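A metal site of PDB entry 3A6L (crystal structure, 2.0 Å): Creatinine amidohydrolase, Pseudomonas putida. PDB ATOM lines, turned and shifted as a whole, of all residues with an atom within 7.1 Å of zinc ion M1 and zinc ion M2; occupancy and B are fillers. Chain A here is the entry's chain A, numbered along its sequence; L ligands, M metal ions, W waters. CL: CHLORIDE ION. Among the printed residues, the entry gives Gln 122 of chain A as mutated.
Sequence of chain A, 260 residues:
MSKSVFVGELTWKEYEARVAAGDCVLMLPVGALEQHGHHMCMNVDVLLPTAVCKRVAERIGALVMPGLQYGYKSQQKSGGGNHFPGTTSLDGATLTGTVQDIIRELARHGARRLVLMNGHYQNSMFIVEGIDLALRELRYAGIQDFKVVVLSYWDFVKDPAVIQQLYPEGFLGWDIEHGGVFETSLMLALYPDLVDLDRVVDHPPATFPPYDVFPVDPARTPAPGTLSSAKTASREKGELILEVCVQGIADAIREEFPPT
The backbone carbonyl oxygen (O) of Glu 34 lies within hydrogen-bond range of a ring nitrogen (ND1) of His 36, at 2.7 Å.
OG of Ser 74 is in hydrogen-bond range of OE2 of Glu 34 (3.0 Å).
The backbone NH of Gly 179 lies within hydrogen-bond range of the side-chain carboxylate of Glu 183.
The side-chain amide nitrogen (NE2) of Gln 122 sits close to a ring nitrogen (NE2) of His 120.
The backbone carbonyl oxygen (O) of Tyr 72 lies within hydrogen-bond range of a ring nitrogen (NE2) of His 120 (2.8 Å).
Within 4 Å of zinc ion M1: Glu 34, Asp 45 and His 120.
Along chain A the residues within 4 Å of zinc ion M1 span positions 34 to 120.
The nearest printed residue that does not touch zinc ion M1 is Tyr 121 (4.3 Å).
Along chain A the residues within 4 Å of zinc ion M2 span positions 36 to 183.
The nearest printed residue that does not touch zinc ion M2 is Val 44 (4.1 Å).
Zinc ion M1 is bound by OE1 of Glu 34 (2.0 Å), OD2 of Asp 45 (2.0 Å) and ND1 of His 120 (2.2 Å).
Zinc ion M1 has three donor atoms within binding distance.
Slightly farther from zinc ion M1 lies CL of the ligand (3.0 Å).
Zinc ion M2 is bound by the side-chain carboxylate (OD1) of Asp 45 (2.1 Å), a ring nitrogen (NE2) of His 36 (2.1 Å) and the side-chain carboxylate (OE2) of Glu 183 (2.2 Å).
Slightly farther from zinc ion M2 lies the side-chain carboxylate (OE1) of Glu 183 (2.6 Å).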
ATOM      1  N   GLY A  31      29.673 -12.432   2.486  1.00  0.00           N
ATOM      2  CA  GLY A  31      28.582 -11.652   3.035  1.00  0.00           C
ATOM      3  C   GLY A  31      27.429 -12.423   3.657  1.00  0.00           C
ATOM      4  O   GLY A  31      27.627 -13.348   4.451  1.00  0.00           O
ATOM      5  N   ALA A  32      26.215 -12.020   3.284  1.00  0.00           N
ATOM      6  CA  ALA A  32      24.991 -12.629   3.789  1.00  0.00           C
ATOM      7  C   ALA A  32      23.763 -11.952   3.182  1.00  0.00           C
ATOM      8  O   ALA A  32      23.862 -10.859   2.639  1.00  0.00           O
ATOM      9  CB  ALA A  32      24.939 -12.501   5.297  1.00  0.00           C
ATOM     10  N   LEU A  33      22.623 -12.635   3.262  1.00  0.00           N
ATOM     11  CA  LEU A  33      21.347 -12.115   2.779  1.00  0.00           C
ATOM     12  C   LEU A  33      20.640 -11.949   4.106  1.00  0.00           C
ATOM     13  O   LEU A  33      20.175 -12.920   4.710  1.00  0.00           O
ATOM     14  CB  LEU A  33      20.609 -13.143   1.904  1.00  0.00           C
ATOM     15  CG  LEU A  33      19.257 -12.671   1.332  1.00  0.00           C
ATOM     16  CD1 LEU A  33      19.510 -11.484   0.410  1.00  0.00           C
ATOM     17  CD2 LEU A  33      18.555 -13.791   0.565  1.00  0.00           C
ATOM     18  N   GLU A  34      20.546 -10.699   4.553  1.00  0.00           N
ATOM     19  CA  GLU A  34      19.977 -10.422   5.855  1.00  0.00           C
ATOM     20  C   GLU A  34      19.149  -9.146   5.885  1.00  0.00           C
ATOM     21  O   GLU A  34      19.479  -8.150   5.234  1.00  0.00           O
ATOM     22  CB  GLU A  34      21.144 -10.317   6.840  1.00  0.00           C
ATOM     23  CG  GLU A  34      20.832  -9.935   8.268  1.00  0.00           C
ATOM     24  CD  GLU A  34      22.118  -9.678   9.042  1.00  0.00           C
ATOM     25  OE1 GLU A  34      22.951  -8.909   8.533  1.00  0.00           O
ATOM     26  OE2 GLU A  34      22.304 -10.233  10.148  1.00  0.00           O
ATOM     27  N   GLN A  35      18.063  -9.180   6.637  1.00  0.00           N
ATOM     28  CA  GLN A  35      17.207  -8.010   6.759  1.00  0.00           C
ATOM     29  C   GLN A  35      18.040  -6.830   7.232  1.00  0.00           C
ATOM     30  O   GLN A  35      18.899  -6.985   8.108  1.00  0.00           O
ATOM     31  CB  GLN A  35      16.084  -8.273   7.784  1.00  0.00           C
ATOM     32  CG  GLN A  35      16.524  -8.383   9.262  1.00  0.00           C
ATOM     33  CD  GLN A  35      16.827  -7.042   9.925  1.00  0.00           C
ATOM     34  OE1 GLN A  35      16.339  -6.004   9.498  1.00  0.00           O
ATOM     35  NE2 GLN A  35      17.628  -7.074  10.986  1.00  0.00           N
ATOM     36  N   HIS A  36      17.807  -5.658   6.648  1.00  0.00           N
ATOM     37  CA  HIS A  36      18.497  -4.447   7.083  1.00  0.00           C
ATOM     38  C   HIS A  36      17.513  -3.299   7.259  1.00  0.00           C
ATOM     39  O   HIS A  36      17.687  -2.231   6.683  1.00  0.00           O
ATOM     40  CB  HIS A  36      19.584  -4.039   6.077  1.00  0.00           C
ATOM     41  CG  HIS A  36      20.878  -4.774   6.263  1.00  0.00           C
ATOM     42  ND1 HIS A  36      21.054  -6.088   5.879  1.00  0.00           N
ATOM     43  CD2 HIS A  36      22.065  -4.392   6.796  1.00  0.00           C
ATOM     44  CE1 HIS A  36      22.278  -6.477   6.160  1.00  0.00           C
ATOM     45  NE2 HIS A  36      22.915  -5.465   6.715  1.00  0.00           N
ATOM     46  N   MET A  40      16.625  -0.241   3.740  1.00  0.00           N
ATOM     47  CA  MET A  40      17.667  -0.815   2.890  1.00  0.00           C
ATOM     48  C   MET A  40      17.370  -2.239   2.424  1.00  0.00           C
ATOM     49  O   MET A  40      16.627  -2.966   3.064  1.00  0.00           O
ATOM     50  CB  MET A  40      19.015  -0.822   3.606  1.00  0.00           C
ATOM     51  CG  MET A  40      19.652   0.521   3.840  1.00  0.00           C
ATOM     52  SD  MET A  40      21.425   0.346   4.170  1.00  0.00           S
ATOM     53  CE  MET A  40      21.421  -0.275   5.848  1.00  0.00           C
ATOM     54  N   VAL A  44      22.983  -6.060   1.441  1.00  0.00           N
ATOM     55  CA  VAL A  44      23.969  -5.102   1.909  1.00  0.00           C
ATOM     56  C   VAL A  44      25.312  -5.745   2.270  1.00  0.00           C
ATOM     57  O   VAL A  44      26.359  -5.289   1.832  1.00  0.00           O
ATOM     58  CB  VAL A  44      23.454  -4.332   3.151  1.00  0.00           C
ATOM     59  CG1 VAL A  44      24.568  -3.523   3.782  1.00  0.00           C
ATOM     60  CG2 VAL A  44      22.292  -3.425   2.762  1.00  0.00           C
ATOM     61  N   ASP A  45      25.268  -6.812   3.082  1.00  0.00           N
ATOM     62  CA  ASP A  45      26.474  -7.507   3.525  1.00  0.00           C
ATOM     63  C   ASP A  45      27.324  -8.103   2.429  1.00  0.00           C
ATOM     64  O   ASP A  45      28.475  -8.466   2.678  1.00  0.00           O
ATOM     65  CB  ASP A  45      26.135  -8.569   4.570  1.00  0.00           C
ATOM     66  CG  ASP A  45      25.654  -7.972   5.868  1.00  0.00           C
ATOM     67  OD1 ASP A  45      25.797  -6.761   6.042  1.00  0.00           O
ATOM     68  OD2 ASP A  45      25.137  -8.713   6.725  1.00  0.00           O
ATOM     69  N   VAL A  46      26.775  -8.238   1.222  1.00  0.00           N
ATOM     70  CA  VAL A  46      27.537  -8.743   0.096  1.00  0.00           C
ATOM     71  C   VAL A  46      28.005  -7.544  -0.734  1.00  0.00           C
ATOM     72  O   VAL A  46      29.179  -7.455  -1.118  1.00  0.00           O
ATOM     73  CB  VAL A  46      26.712  -9.680  -0.824  1.00  0.00           C
ATOM     74  CG1 VAL A  46      27.525 -10.014  -2.073  1.00  0.00           C
ATOM     75  CG2 VAL A  46      26.347 -10.951  -0.099  1.00  0.00           C
ATOM     76  N   LEU A  48      28.572  -4.312   0.035  1.00  0.00           N
ATOM     77  CA  LEU A  48      29.620  -3.484   0.611  1.00  0.00           C
ATOM     78  C   LEU A  48      31.022  -4.096   0.597  1.00  0.00           C
ATOM     79  O   LEU A  48      31.961  -3.456   0.134  1.00  0.00           O
ATOM     80  CB  LEU A  48      29.238  -3.081   2.035  1.00  0.00           C
ATOM     81  CG  LEU A  48      27.921  -2.291   2.123  1.00  0.00           C
ATOM     82  CD1 LEU A  48      27.735  -1.827   3.539  1.00  0.00           C
ATOM     83  CD2 LEU A  48      27.939  -1.093   1.170  1.00  0.00           C
ATOM     84  N   TYR A  72      26.578 -16.922   7.855  1.00  0.00           N
ATOM     85  CA  TYR A  72      26.070 -17.561   9.044  1.00  0.00           C
ATOM     86  C   TYR A  72      24.842 -16.870   9.612  1.00  0.00           C
ATOM     87  O   TYR A  72      24.537 -15.717   9.291  1.00  0.00           O
ATOM     88  CB  TYR A  72      27.160 -17.657  10.115  1.00  0.00           C
ATOM     89  CG  TYR A  72      26.722 -18.447  11.323  1.00  0.00           C
ATOM     90  CD1 TYR A  72      26.383 -19.796  11.220  1.00  0.00           C
ATOM     91  CD2 TYR A  72      26.579 -17.819  12.559  1.00  0.00           C
ATOM     92  CE1 TYR A  72      25.890 -20.500  12.329  1.00  0.00           C
ATOM     93  CE2 TYR A  72      26.107 -18.518  13.672  1.00  0.00           C
ATOM     94  CZ  TYR A  72      25.758 -19.843  13.552  1.00  0.00           C
ATOM     95  OH  TYR A  72      25.278 -20.506  14.663  1.00  0.00           O
ATOM     96  N   SER A  74      22.066 -14.916  11.554  1.00  0.00           N
ATOM     97  CA  SER A  74      22.024 -13.583  12.119  1.00  0.00           C
ATOM     98  C   SER A  74      21.803 -13.652  13.624  1.00  0.00           C
ATOM     99  O   SER A  74      20.874 -14.309  14.098  1.00  0.00           O
ATOM    100  CB  SER A  74      20.881 -12.795  11.472  1.00  0.00           C
ATOM    101  OG  SER A  74      20.592 -11.618  12.197  1.00  0.00           O
ATOM    102  N   SER A  78      23.527  -8.633  17.229  1.00  0.00           N
ATOM    103  CA  SER A  78      24.463  -8.278  16.177  1.00  0.00           C
ATOM    104  C   SER A  78      23.748  -7.877  14.904  1.00  0.00           C
ATOM    105  O   SER A  78      24.162  -6.929  14.224  1.00  0.00           O
ATOM    106  CB  SER A  78      25.411  -9.448  15.895  1.00  0.00           C
ATOM    107  N   GLY A  79      22.679  -8.576  14.566  1.00  0.00           N
ATOM    108  CA  GLY A  79      21.964  -8.259  13.349  1.00  0.00           C
ATOM    109  C   GLY A  79      20.459  -8.372  13.438  1.00  0.00           C
ATOM    110  O   GLY A  79      19.808  -8.522  12.405  1.00  0.00           O
ATOM    111  N   GLY A 119      31.766  -9.215   5.547  1.00  0.00           N
ATOM    112  CA  GLY A 119      30.848  -8.091   5.613  1.00  0.00           C
ATOM    113  C   GLY A 119      29.647  -8.384   6.507  1.00  0.00           C
ATOM    114  O   GLY A 119      28.729  -7.557   6.620  1.00  0.00           O
ATOM    115  N   HIS A 120      29.644  -9.545   7.140  1.00  0.00           N
ATOM    116  CA  HIS A 120      28.562  -9.971   8.028  1.00  0.00           C
ATOM    117  C   HIS A 120      29.155 -10.368   9.386  1.00  0.00           C
ATOM    118  O   HIS A 120      29.914 -11.336   9.484  1.00  0.00           O
ATOM    119  CB  HIS A 120      27.809 -11.148   7.382  1.00  0.00           C
ATOM    120  CG  HIS A 120      26.777 -11.791   8.256  1.00  0.00           C
ATOM    121  ND1 HIS A 120      25.655 -11.128   8.709  1.00  0.00           N
ATOM    122  CD2 HIS A 120      26.689 -13.052   8.751  1.00  0.00           C
ATOM    123  CE1 HIS A 120      24.924 -11.950   9.437  1.00  0.00           C
ATOM    124  NE2 HIS A 120      25.526 -13.125   9.472  1.00  0.00           N
ATOM    125  N   TYR A 121      28.806  -9.607  10.409  1.00  0.00           N
ATOM    126  CA  TYR A 121      29.298  -9.781  11.774  1.00  0.00           C
ATOM    127  C   TYR A 121      29.571 -11.215  12.290  1.00  0.00           C
ATOM    128  O   TYR A 121      30.673 -11.524  12.764  1.00  0.00           O
ATOM    129  CB  TYR A 121      28.319  -9.089  12.737  1.00  0.00           C
ATOM    130  CG  TYR A 121      28.988  -8.533  13.969  1.00  0.00           C
ATOM    131  CD1 TYR A 121      29.857  -7.451  13.877  1.00  0.00           C
ATOM    132  CD2 TYR A 121      28.757  -9.098  15.228  1.00  0.00           C
ATOM    133  CE1 TYR A 121      30.500  -6.939  15.007  1.00  0.00           C
ATOM    134  CE2 TYR A 121      29.400  -8.593  16.364  1.00  0.00           C
ATOM    135  CZ  TYR A 121      30.265  -7.515  16.236  1.00  0.00           C
ATOM    136  OH  TYR A 121      30.915  -7.016  17.350  1.00  0.00           O
ATOM    137  N   GLN A 122      28.577 -12.080  12.190  1.00  0.00           N
ATOM    138  CA  GLN A 122      28.713 -13.441  12.686  1.00  0.00           C
ATOM    139  C   GLN A 122      29.529 -14.443  11.850  1.00  0.00           C
ATOM    140  O   GLN A 122      29.739 -15.564  12.292  1.00  0.00           O
ATOM    141  CB  GLN A 122      27.319 -14.024  12.940  1.00  0.00           C
ATOM    142  CG  GLN A 122      26.395 -13.141  13.803  1.00  0.00           C
ATOM    143  CD  GLN A 122      25.742 -11.995  13.020  1.00  0.00           C
ATOM    144  OE1 GLN A 122      24.703 -11.463  13.421  1.00  0.00           O
ATOM    145  NE2 GLN A 122      26.350 -11.594  11.902  1.00  0.00           N
ATOM    146  N   ASN A 123      29.986 -14.050  10.662  1.00  0.00           N
ATOM    147  CA  ASN A 123      30.747 -14.982   9.818  1.00  0.00           C
ATOM    148  C   ASN A 123      32.135 -15.392  10.308  1.00  0.00           C
ATOM    149  O   ASN A 123      32.552 -16.544  10.136  1.00  0.00           O
ATOM    150  CB  ASN A 123      30.948 -14.427   8.404  1.00  0.00           C
ATOM    151  CG  ASN A 123      29.671 -14.396   7.589  1.00  0.00           C
ATOM    152  OD1 ASN A 123      28.747 -15.167   7.843  1.00  0.00           O
ATOM    153  ND2 ASN A 123      29.627 -13.516   6.595  1.00  0.00           N
ATOM    154  N   TYR A 153      35.983  -5.437   7.125  1.00  0.00           N
ATOM    155  CA  TYR A 153      36.307  -4.082   6.678  1.00  0.00           C
ATOM    156  C   TYR A 153      35.992  -2.955   7.644  1.00  0.00           C
ATOM    157  O   TYR A 153      36.653  -1.924   7.619  1.00  0.00           O
ATOM    158  CB  TYR A 153      35.661  -3.821   5.311  1.00  0.00           C
ATOM    159  CG  TYR A 153      34.166  -3.601   5.335  1.00  0.00           C
ATOM    160  CD1 TYR A 153      33.647  -2.326   5.581  1.00  0.00           C
ATOM    161  CD2 TYR A 153      33.277  -4.653   5.147  1.00  0.00           C
ATOM    162  CE1 TYR A 153      32.266  -2.120   5.634  1.00  0.00           C
ATOM    163  CE2 TYR A 153      31.894  -4.453   5.192  1.00  0.00           C
ATOM    164  CZ  TYR A 153      31.404  -3.181   5.435  1.00  0.00           C
ATOM    165  OH  TYR A 153      30.047  -2.949   5.502  1.00  0.00           O
ATOM    166  N   TRP A 154      34.989  -3.121   8.502  1.00  0.00           N
ATOM    167  CA  TRP A 154      34.656  -2.053   9.442  1.00  0.00           C
ATOM    168  C   TRP A 154      35.694  -1.847  10.538  1.00  0.00           C
ATOM    169  O   TRP A 154      35.737  -0.785  11.164  1.00  0.00           O
ATOM    170  CB  TRP A 154      33.265  -2.287  10.064  1.00  0.00           C
ATOM    171  CG  TRP A 154      33.084  -3.593  10.743  1.00  0.00           C
ATOM    172  CD1 TRP A 154      33.518  -3.936  11.996  1.00  0.00           C
ATOM    173  CD2 TRP A 154      32.447  -4.748  10.201  1.00  0.00           C
ATOM    174  NE1 TRP A 154      33.176  -5.242  12.263  1.00  0.00           N
ATOM    175  CE2 TRP A 154      32.527  -5.773  11.175  1.00  0.00           C
ATOM    176  CE3 TRP A 154      31.821  -5.031   8.972  1.00  0.00           C
ATOM    177  CZ2 TRP A 154      31.990  -7.042  10.967  1.00  0.00           C
ATOM    178  CZ3 TRP A 154      31.295  -6.310   8.770  1.00  0.00           C
ATOM    179  CH2 TRP A 154      31.380  -7.293   9.762  1.00  0.00           C
ATOM    180  N   GLU A 177      25.583  -1.485  15.326  1.00  0.00           N
ATOM    181  CA  GLU A 177      25.575  -0.747  14.062  1.00  0.00           C
ATOM    182  C   GLU A 177      24.966  -1.585  12.943  1.00  0.00           C
ATOM    183  O   GLU A 177      25.526  -1.675  11.855  1.00  0.00           O
ATOM    184  CB  GLU A 177      26.995  -0.351  13.655  1.00  0.00           C
ATOM    185  CG  GLU A 177      27.384   1.096  13.942  1.00  0.00           C
ATOM    186  CD  GLU A 177      26.586   2.117  13.132  1.00  0.00           C
ATOM    187  OE1 GLU A 177      26.143   1.798  12.015  1.00  0.00           O
ATOM    188  OE2 GLU A 177      26.427   3.255  13.616  1.00  0.00           O
ATOM    189  N   HIS A 178      23.832  -2.222  13.206  1.00  0.00           N
ATOM    190  CA  HIS A 178      23.186  -3.014  12.161  1.00  0.00           C
ATOM    191  C   HIS A 178      22.156  -2.147  11.467  1.00  0.00           C
ATOM    192  O   HIS A 178      21.149  -1.759  12.071  1.00  0.00           O
ATOM    193  CB  HIS A 178      22.493  -4.261  12.745  1.00  0.00           C
ATOM    194  CG  HIS A 178      21.775  -5.074  11.705  1.00  0.00           C
ATOM    195  ND1 HIS A 178      22.437  -5.800  10.738  1.00  0.00           N
ATOM    196  CD2 HIS A 178      20.458  -5.237  11.461  1.00  0.00           C
ATOM    197  CE1 HIS A 178      21.555  -6.371   9.936  1.00  0.00           C
ATOM    198  NE2 HIS A 178      20.339  -6.037  10.349  1.00  0.00           N
ATOM    199  N   GLY A 179      22.403  -1.838  10.192  1.00  0.00           N
ATOM    200  CA  GLY A 179      21.482  -1.018   9.424  1.00  0.00           C
ATOM    201  C   GLY A 179      21.442   0.414   9.935  1.00  0.00           C
ATOM    202  O   GLY A 179      20.448   1.113   9.749  1.00  0.00           O
ATOM    203  N   GLU A 183      26.557   1.492   7.743  1.00  0.00           N
ATOM    204  CA  GLU A 183      26.163   0.837   6.513  1.00  0.00           C
ATOM    205  C   GLU A 183      25.301   1.708   5.615  1.00  0.00           C
ATOM    206  O   GLU A 183      25.511   1.729   4.400  1.00  0.00           O
ATOM    207  CB  GLU A 183      25.451  -0.473   6.814  1.00  0.00           C
ATOM    208  CG  GLU A 183      26.371  -1.509   7.380  1.00  0.00           C
ATOM    209  CD  GLU A 183      25.714  -2.848   7.485  1.00  0.00           C
ATOM    210  OE1 GLU A 183      24.677  -2.944   8.176  1.00  0.00           O
ATOM    211  OE2 GLU A 183      26.236  -3.800   6.859  1.00  0.00           O
HETATM  212 CL    CL L   1      25.829  -6.685  10.325  1.00  0.00          CL
HETATM  213 ZN    ZN M   1      24.939  -9.044   8.685  1.00  0.00          ZN
HETATM  214 ZN    ZN M   2      24.897  -5.452   7.399  1.00  0.00          ZN
HETATM  215  O   HOH W   1      24.184  -9.209  11.620  1.00  0.00           O
